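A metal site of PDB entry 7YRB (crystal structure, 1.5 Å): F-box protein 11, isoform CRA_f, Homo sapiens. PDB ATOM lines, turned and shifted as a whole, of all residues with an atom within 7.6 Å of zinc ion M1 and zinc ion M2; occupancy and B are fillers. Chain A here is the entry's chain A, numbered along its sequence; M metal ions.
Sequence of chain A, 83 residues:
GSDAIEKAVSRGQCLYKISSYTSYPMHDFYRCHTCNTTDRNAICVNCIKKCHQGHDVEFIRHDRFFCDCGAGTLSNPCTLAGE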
ATOM      1  N   GLN A  13       7.503 -19.297 -18.730  1.00  0.00           N
ATOM      2  CA  GLN A  13       8.355 -18.873 -19.825  1.00  0.00           C
ATOM      3  C   GLN A  13       8.871 -17.457 -19.547  1.00  0.00           C
ATOM      4  O   GLN A  13       8.373 -16.723 -18.686  1.00  0.00           O
ATOM      5  CB  GLN A  13       7.583 -18.965 -21.149  1.00  0.00           C
ATOM      6  CG  GLN A  13       7.256 -20.389 -21.744  1.00  0.00           C
ATOM      7  CD  GLN A  13       8.354 -21.482 -21.640  1.00  0.00           C
ATOM      8  OE1 GLN A  13       9.467 -21.340 -22.153  1.00  0.00           O
ATOM      9  NE2 GLN A  13       7.988 -22.621 -21.020  1.00  0.00           N
ATOM     10  N   CYS A  14       9.894 -17.068 -20.302  1.00  0.00           N
ATOM     11  CA  CYS A  14      10.388 -15.707 -20.228  1.00  0.00           C
ATOM     12  C   CYS A  14       9.506 -14.748 -21.018  1.00  0.00           C
ATOM     13  O   CYS A  14       9.101 -15.040 -22.157  1.00  0.00           O
ATOM     14  CB  CYS A  14      11.810 -15.612 -20.773  1.00  0.00           C
ATOM     15  SG  CYS A  14      12.502 -13.894 -20.913  1.00  0.00           S
ATOM     16  N   LEU A  15       9.206 -13.607 -20.430  1.00  0.00           N
ATOM     17  CA  LEU A  15       8.300 -12.673 -21.084  1.00  0.00           C
ATOM     18  C   LEU A  15       8.879 -12.048 -22.349  1.00  0.00           C
ATOM     19  O   LEU A  15       8.128 -11.451 -23.132  1.00  0.00           O
ATOM     20  CB  LEU A  15       7.902 -11.589 -20.109  1.00  0.00           C
ATOM     21  CG  LEU A  15       6.956 -12.025 -18.993  1.00  0.00           C
ATOM     22  CD1 LEU A  15       6.629 -10.895 -18.073  1.00  0.00           C
ATOM     23  CD2 LEU A  15       5.652 -12.622 -19.549  1.00  0.00           C
ATOM     24  N   TYR A  16      10.179 -12.153 -22.585  1.00  0.00           N
ATOM     25  CA  TYR A  16      10.724 -11.627 -23.828  1.00  0.00           C
ATOM     26  C   TYR A  16      10.150 -12.343 -25.037  1.00  0.00           C
ATOM     27  O   TYR A  16      10.113 -11.768 -26.136  1.00  0.00           O
ATOM     28  CB  TYR A  16      12.241 -11.740 -23.784  1.00  0.00           C
ATOM     29  CG  TYR A  16      12.931 -11.029 -24.904  1.00  0.00           C
ATOM     30  CD1 TYR A  16      13.129  -9.657 -24.850  1.00  0.00           C
ATOM     31  CD2 TYR A  16      13.397 -11.722 -25.994  1.00  0.00           C
ATOM     32  CE1 TYR A  16      13.767  -9.011 -25.865  1.00  0.00           C
ATOM     33  CE2 TYR A  16      14.044 -11.074 -27.019  1.00  0.00           C
ATOM     34  CZ  TYR A  16      14.224  -9.709 -26.953  1.00  0.00           C
ATOM     35  OH  TYR A  16      14.874  -9.046 -27.973  1.00  0.00           O
ATOM     36  N   LYS A  17       9.704 -13.583 -24.875  1.00  0.00           N
ATOM     37  CA  LYS A  17       9.167 -14.362 -25.986  1.00  0.00           C
ATOM     38  C   LYS A  17       7.855 -13.802 -26.497  1.00  0.00           C
ATOM     39  O   LYS A  17       7.388 -14.217 -27.574  1.00  0.00           O
ATOM     40  CB  LYS A  17       8.944 -15.816 -25.577  1.00  0.00           C
ATOM     41  CG  LYS A  17      10.208 -16.590 -25.258  1.00  0.00           C
ATOM     42  CD  LYS A  17      11.135 -16.748 -26.450  1.00  0.00           C
ATOM     43  CE  LYS A  17      12.316 -17.608 -25.999  1.00  0.00           C
ATOM     44  NZ  LYS A  17      13.194 -18.089 -27.090  1.00  0.00           N
ATOM     45  N   ALA A  42      16.359  -5.058 -15.990  1.00  0.00           N
ATOM     46  CA  ALA A  42      15.012  -5.473 -15.593  1.00  0.00           C
ATOM     47  C   ALA A  42      14.811  -6.903 -16.052  1.00  0.00           C
ATOM     48  O   ALA A  42      15.022  -7.217 -17.226  1.00  0.00           O
ATOM     49  CB  ALA A  42      13.942  -4.588 -16.218  1.00  0.00           C
ATOM     50  N   ILE A  43      14.478  -7.786 -15.107  1.00  0.00           N
ATOM     51  CA  ILE A  43      14.406  -9.225 -15.344  1.00  0.00           C
ATOM     52  C   ILE A  43      13.046  -9.755 -14.907  1.00  0.00           C
ATOM     53  O   ILE A  43      12.549  -9.404 -13.824  1.00  0.00           O
ATOM     54  CB  ILE A  43      15.548  -9.962 -14.609  1.00  0.00           C
ATOM     55  CG1 ILE A  43      16.906  -9.393 -15.070  1.00  0.00           C
ATOM     56  CG2 ILE A  43      15.484 -11.465 -14.801  1.00  0.00           C
ATOM     57  CD1 ILE A  43      18.109  -9.963 -14.317  1.00  0.00           C
ATOM     58  N   CYS A  44      12.458 -10.634 -15.719  1.00  0.00           N
ATOM     59  CA  CYS A  44      11.138 -11.168 -15.417  1.00  0.00           C
ATOM     60  C   CYS A  44      11.226 -12.205 -14.290  1.00  0.00           C
ATOM     61  O   CYS A  44      12.300 -12.683 -13.926  1.00  0.00           O
ATOM     62  CB  CYS A  44      10.518 -11.771 -16.679  1.00  0.00           C
ATOM     63  SG  CYS A  44      11.099 -13.390 -17.222  1.00  0.00           S
ATOM     64  N   VAL A  45      10.059 -12.521 -13.696  1.00  0.00           N
ATOM     65  CA  VAL A  45      10.086 -13.343 -12.488  1.00  0.00           C
ATOM     66  C   VAL A  45      10.570 -14.762 -12.778  1.00  0.00           C
ATOM     67  O   VAL A  45      11.262 -15.367 -11.954  1.00  0.00           O
ATOM     68  CB  VAL A  45       8.705 -13.373 -11.805  1.00  0.00           C
ATOM     69  CG1 VAL A  45       7.689 -14.057 -12.688  1.00  0.00           C
ATOM     70  CG2 VAL A  45       8.806 -14.028 -10.409  1.00  0.00           C
ATOM     71  N   ASN A  46      10.245 -15.316 -13.958  1.00  0.00           N
ATOM     72  CA  ASN A  46      10.695 -16.685 -14.224  1.00  0.00           C
ATOM     73  C   ASN A  46      12.192 -16.726 -14.441  1.00  0.00           C
ATOM     74  O   ASN A  46      12.841 -17.686 -13.992  1.00  0.00           O
ATOM     75  CB  ASN A  46       9.941 -17.258 -15.419  1.00  0.00           C
ATOM     76  CG  ASN A  46       8.498 -17.574 -15.062  1.00  0.00           C
ATOM     77  OD1 ASN A  46       8.225 -18.020 -13.941  1.00  0.00           O
ATOM     78  ND2 ASN A  46       7.575 -17.306 -15.981  1.00  0.00           N
ATOM     79  N   CYS A  47      12.760 -15.710 -15.091  1.00  0.00           N
ATOM     80  CA  CYS A  47      14.207 -15.641 -15.232  1.00  0.00           C
ATOM     81  C   CYS A  47      14.891 -15.428 -13.902  1.00  0.00           C
ATOM     82  O   CYS A  47      15.932 -16.057 -13.625  1.00  0.00           O
ATOM     83  CB  CYS A  47      14.567 -14.516 -16.197  1.00  0.00           C
ATOM     84  SG  CYS A  47      14.317 -14.950 -17.916  1.00  0.00           S
ATOM     85  N   ILE A  48      14.337 -14.588 -13.028  1.00  0.00           N
ATOM     86  CA  ILE A  48      15.046 -14.335 -11.764  1.00  0.00           C
ATOM     87  C   ILE A  48      15.112 -15.595 -10.920  1.00  0.00           C
ATOM     88  O   ILE A  48      16.076 -15.794 -10.173  1.00  0.00           O
ATOM     89  CB  ILE A  48      14.411 -13.147 -11.007  1.00  0.00           C
ATOM     90  CG1 ILE A  48      15.487 -12.387 -10.213  1.00  0.00           C
ATOM     91  CG2 ILE A  48      13.262 -13.608 -10.117  1.00  0.00           C
ATOM     92  CD1 ILE A  48      16.511 -11.676 -11.092  1.00  0.00           C
ATOM     93  N   LYS A  50      15.081 -18.783 -12.116  1.00  0.00           N
ATOM     94  CA  LYS A  50      15.788 -19.884 -12.762  1.00  0.00           C
ATOM     95  C   LYS A  50      17.156 -19.454 -13.280  1.00  0.00           C
ATOM     96  O   LYS A  50      18.188 -19.955 -12.815  1.00  0.00           O
ATOM     97  CB  LYS A  50      14.916 -20.457 -13.899  1.00  0.00           C
ATOM     98  CG  LYS A  50      15.519 -21.666 -14.565  1.00  0.00           C
ATOM     99  CD  LYS A  50      14.482 -22.514 -15.263  1.00  0.00           C
ATOM    100  CE  LYS A  50      15.103 -23.851 -15.649  1.00  0.00           C
ATOM    101  NZ  LYS A  50      15.982 -23.689 -16.830  1.00  0.00           N
ATOM    102  N   CYS A  51      17.205 -18.479 -14.176  1.00  0.00           N
ATOM    103  CA  CYS A  51      18.459 -17.996 -14.729  1.00  0.00           C
ATOM    104  C   CYS A  51      19.332 -17.325 -13.690  1.00  0.00           C
ATOM    105  O   CYS A  51      20.565 -17.233 -13.883  1.00  0.00           O
ATOM    106  CB  CYS A  51      18.177 -17.004 -15.861  1.00  0.00           C
ATOM    107  SG  CYS A  51      16.955 -17.624 -17.053  1.00  0.00           S
ATOM    108  N   HIS A  52      18.753 -16.824 -12.602  1.00  0.00           N
ATOM    109  CA  HIS A  52      19.517 -16.109 -11.595  1.00  0.00           C
ATOM    110  C   HIS A  52      19.351 -16.723 -10.216  1.00  0.00           C
ATOM    111  O   HIS A  52      19.516 -16.048  -9.205  1.00  0.00           O
ATOM    112  CB  HIS A  52      19.163 -14.629 -11.607  1.00  0.00           C
ATOM    113  CG  HIS A  52      19.353 -14.052 -12.960  1.00  0.00           C
ATOM    114  ND1 HIS A  52      20.537 -13.517 -13.397  1.00  0.00           N
ATOM    115  CD2 HIS A  52      18.485 -13.959 -14.005  1.00  0.00           C
ATOM    116  CE1 HIS A  52      20.394 -13.102 -14.647  1.00  0.00           C
ATOM    117  NE2 HIS A  52      19.165 -13.395 -15.042  1.00  0.00           N
ATOM    118  N   PHE A  65       8.141  -3.210 -18.674  1.00  0.00           N
ATOM    119  CA  PHE A  65       9.538  -3.540 -18.941  1.00  0.00           C
ATOM    120  C   PHE A  65       9.568  -4.559 -20.065  1.00  0.00           C
ATOM    121  O   PHE A  65       8.559  -5.207 -20.355  1.00  0.00           O
ATOM    122  CB  PHE A  65      10.238  -4.064 -17.667  1.00  0.00           C
ATOM    123  CG  PHE A  65       9.897  -5.482 -17.298  1.00  0.00           C
ATOM    124  CD1 PHE A  65       8.667  -5.778 -16.746  1.00  0.00           C
ATOM    125  CD2 PHE A  65      10.800  -6.501 -17.464  1.00  0.00           C
ATOM    126  CE1 PHE A  65       8.336  -7.075 -16.399  1.00  0.00           C
ATOM    127  CE2 PHE A  65      10.479  -7.810 -17.100  1.00  0.00           C
ATOM    128  CZ  PHE A  65       9.257  -8.084 -16.566  1.00  0.00           C
ATOM    129  N   PHE A  66      10.764  -4.786 -20.614  1.00  0.00           N
ATOM    130  CA  PHE A  66      11.051  -6.018 -21.320  1.00  0.00           C
ATOM    131  C   PHE A  66      12.275  -6.655 -20.680  1.00  0.00           C
ATOM    132  O   PHE A  66      13.175  -5.959 -20.158  1.00  0.00           O
ATOM    133  CB  PHE A  66      11.217  -5.819 -22.848  1.00  0.00           C
ATOM    134  CG  PHE A  66      12.479  -5.108 -23.269  1.00  0.00           C
ATOM    135  CD1 PHE A  66      13.695  -5.756 -23.284  1.00  0.00           C
ATOM    136  CD2 PHE A  66      12.438  -3.781 -23.689  1.00  0.00           C
ATOM    137  CE1 PHE A  66      14.850  -5.116 -23.686  1.00  0.00           C
ATOM    138  CE2 PHE A  66      13.592  -3.140 -24.091  1.00  0.00           C
ATOM    139  CZ  PHE A  66      14.795  -3.803 -24.091  1.00  0.00           C
ATOM    140  N   CYS A  67      12.293  -7.987 -20.684  1.00  0.00           N
ATOM    141  CA  CYS A  67      13.242  -8.751 -19.875  1.00  0.00           C
ATOM    142  C   CYS A  67      14.635  -8.732 -20.511  1.00  0.00           C
ATOM    143  O   CYS A  67      14.831  -9.271 -21.606  1.00  0.00           O
ATOM    144  CB  CYS A  67      12.773 -10.198 -19.704  1.00  0.00           C
ATOM    145  SG  CYS A  67      13.921 -11.148 -18.702  1.00  0.00           S
ATOM    146  N   ASP A  68      15.607  -8.123 -19.817  1.00  0.00           N
ATOM    147  CA  ASP A  68      16.977  -8.070 -20.328  1.00  0.00           C
ATOM    148  C   ASP A  68      17.665  -9.428 -20.331  1.00  0.00           C
ATOM    149  O   ASP A  68      18.631  -9.626 -21.082  1.00  0.00           O
ATOM    150  CB  ASP A  68      17.795  -7.080 -19.490  1.00  0.00           C
ATOM    151  CG  ASP A  68      17.365  -5.660 -19.698  1.00  0.00           C
ATOM    152  OD1 ASP A  68      16.996  -5.329 -20.844  1.00  0.00           O
ATOM    153  OD2 ASP A  68      17.373  -4.877 -18.733  1.00  0.00           O
ATOM    154  N   CYS A  69      17.243 -10.363 -19.479  1.00  0.00           N
ATOM    155  CA  CYS A  69      17.797 -11.719 -19.522  1.00  0.00           C
ATOM    156  C   CYS A  69      17.460 -12.390 -20.830  1.00  0.00           C
ATOM    157  O   CYS A  69      18.340 -12.845 -21.569  1.00  0.00           O
ATOM    158  CB  CYS A  69      17.290 -12.534 -18.323  1.00  0.00           C
ATOM    159  SG  CYS A  69      18.074 -14.109 -18.084  1.00  0.00           S
ATOM    160  N   GLY A  70      16.172 -12.420 -21.184  1.00  0.00           N
ATOM    161  CA  GLY A  70      15.758 -13.019 -22.437  1.00  0.00           C
ATOM    162  C   GLY A  70      16.270 -12.280 -23.651  1.00  0.00           C
ATOM    163  O   GLY A  70      16.483 -12.881 -24.712  1.00  0.00           O
ATOM    164  N   ALA A  71      16.465 -10.968 -23.522  1.00  0.00           N
ATOM    165  CA  ALA A  71      16.995 -10.193 -24.641  1.00  0.00           C
ATOM    166  C   ALA A  71      18.450 -10.531 -24.925  1.00  0.00           C
ATOM    167  O   ALA A  71      18.982 -10.163 -25.984  1.00  0.00           O
ATOM    168  CB  ALA A  71      16.828  -8.701 -24.340  1.00  0.00           C
ATOM    169  N   LEU A  74      22.655  -9.679 -20.729  1.00  0.00           N
ATOM    170  CA  LEU A  74      23.329  -9.860 -19.451  1.00  0.00           C
ATOM    171  C   LEU A  74      24.564 -10.741 -19.584  1.00  0.00           C
ATOM    172  O   LEU A  74      24.775 -11.429 -20.583  1.00  0.00           O
ATOM    173  CB  LEU A  74      22.396 -10.463 -18.403  1.00  0.00           C
ATOM    174  CG  LEU A  74      21.084  -9.715 -18.109  1.00  0.00           C
ATOM    175  CD1 LEU A  74      20.325 -10.456 -17.024  1.00  0.00           C
ATOM    176  CD2 LEU A  74      21.349  -8.289 -17.699  1.00  0.00           C
ATOM    177  N   ASN A  76      25.253 -13.490 -18.572  1.00  0.00           N
ATOM    178  CA  ASN A  76      25.028 -14.923 -18.649  1.00  0.00           C
ATOM    179  C   ASN A  76      23.873 -15.226 -19.599  1.00  0.00           C
ATOM    180  O   ASN A  76      22.983 -14.401 -19.768  1.00  0.00           O
ATOM    181  CB  ASN A  76      24.731 -15.461 -17.251  1.00  0.00           C
ATOM    182  CG  ASN A  76      25.958 -16.079 -16.597  1.00  0.00           C
ATOM    183  OD1 ASN A  76      26.758 -16.729 -17.270  1.00  0.00           O
ATOM    184  ND2 ASN A  76      26.129 -15.841 -15.291  1.00  0.00           N
ATOM    185  N   PRO A  77      23.886 -16.384 -20.260  1.00  0.00           N
ATOM    186  CA  PRO A  77      22.807 -16.677 -21.210  1.00  0.00           C
ATOM    187  C   PRO A  77      21.513 -17.092 -20.514  1.00  0.00           C
ATOM    188  O   PRO A  77      21.519 -17.676 -19.424  1.00  0.00           O
ATOM    189  CB  PRO A  77      23.388 -17.830 -22.046  1.00  0.00           C
ATOM    190  CG  PRO A  77      24.290 -18.551 -21.085  1.00  0.00           C
ATOM    191  CD  PRO A  77      24.886 -17.473 -20.183  1.00  0.00           C
ATOM    192  N   CYS A  78      20.403 -16.767 -21.154  1.00  0.00           N
ATOM    193  CA  CYS A  78      19.096 -17.110 -20.600  1.00  0.00           C
ATOM    194  C   CYS A  78      18.863 -18.619 -20.703  1.00  0.00           C
ATOM    195  O   CYS A  78      18.999 -19.208 -21.772  1.00  0.00           O
ATOM    196  CB  CYS A  78      17.988 -16.354 -21.339  1.00  0.00           C
ATOM    197  SG  CYS A  78      16.327 -16.562 -20.650  1.00  0.00           S
ATOM    198  N   THR A  79      18.485 -19.231 -19.591  1.00  0.00           N
ATOM    199  CA  THR A  79      18.177 -20.655 -19.579  1.00  0.00           C
ATOM    200  C   THR A  79      16.746 -20.961 -19.980  1.00  0.00           C
ATOM    201  O   THR A  79      16.355 -22.132 -19.977  1.00  0.00           O
ATOM    202  CB  THR A  79      18.426 -21.254 -18.206  1.00  0.00           C
ATOM    203  OG1 THR A  79      17.354 -20.872 -17.324  1.00  0.00           O
ATOM    204  CG2 THR A  79      19.752 -20.782 -17.657  1.00  0.00           C
ATOM    205  N   LEU A  80      15.936 -19.938 -20.268  1.00  0.00           N
ATOM    206  CA  LEU A  80      14.572 -20.131 -20.737  1.00  0.00           C
ATOM    207  C   LEU A  80      14.413 -19.854 -22.225  1.00  0.00           C
ATOM    208  O   LEU A  80      13.291 -19.824 -22.718  1.00  0.00           O
ATOM    209  CB  LEU A  80      13.626 -19.225 -19.939  1.00  0.00           C
ATOM    210  CG  LEU A  80      13.410 -19.647 -18.493  1.00  0.00           C
ATOM    211  CD1 LEU A  80      12.720 -18.532 -17.745  1.00  0.00           C
ATOM    212  CD2 LEU A  80      12.560 -20.918 -18.383  1.00  0.00           C
ATOM    213  N   ALA A  81      15.509 -19.628 -22.939  1.00  0.00           N
ATOM    214  CA  ALA A  81      15.438 -19.216 -24.343  1.00  0.00           C
ATOM    215  C   ALA A  81      15.963 -20.277 -25.299  1.00  0.00           C
ATOM    216  O   ALA A  81      16.166 -19.971 -26.481  1.00  0.00           O
ATOM    217  CB  ALA A  81      16.179 -17.896 -24.540  1.00  0.00           C
HETATM  218 ZN    ZN M   1      12.895 -13.245 -18.732  1.00  0.00          ZN
HETATM  219 ZN    ZN M   2      16.453 -15.772 -18.512  1.00  0.00          ZN
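N of Leu 80 lies close to SG of Cys 78, 3.4 Å away.
SG of Cys 14 lies close to N of Tyr 16 (3.4 Å).
The side-chain sulfur (SG) of Cys 67 lies close to the backbone NH (N) of Cys 69 (3.5 Å).
N of Gly 70 sits close to SG of Cys 67, 3.6 Å away.
The backbone NH (N) of Leu 15 sits close to the side-chain sulfur (SG) of Cys 44, at 3.7 Å.
NE2 of His 52 sits close to SG of Cys 69 (3.3 Å).
O of Cys 47 is in hydrogen-bond range of N of His 52 (3.1 Å).
The side-chain hydroxyl (OG1) of Thr 79 sits close to the side-chain sulfur (SG) of Cys 51 (3.3 Å).
Zinc ion M1 is bound by SG of Cys 14 (2.3 Å), SG of Cys 67 (2.3 Å), SG of Cys 44 (2.4 Å) and SG of Cys 47 (2.4 Å).
Within 4 Å of zinc ion M2: Cys 47, Cys 51, Cys 69 and Cys 78.
The nearest printed residue that does not touch zinc ion M2 is Thr 79 (4.2 Å).
Within 4 Å of zinc ion M1: Cys 14, Cys 44, Cys 47 and Cys 67.
The nearest printed residue that does not touch zinc ion M1 is Leu 15 (4.1 Å).
Zinc ion M2 is bound by the side-chain sulfur (SG) of Cys 78 (2.3 Å), the side-chain sulfur (SG) of Cys 69 (2.4 Å), the side-chain sulfur (SG) of Cys 47 (2.4 Å) and the side-chain sulfur (SG) of Cys 51 (2.4 Å).
Zinc ion M2 has four donor atoms within binding distance.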
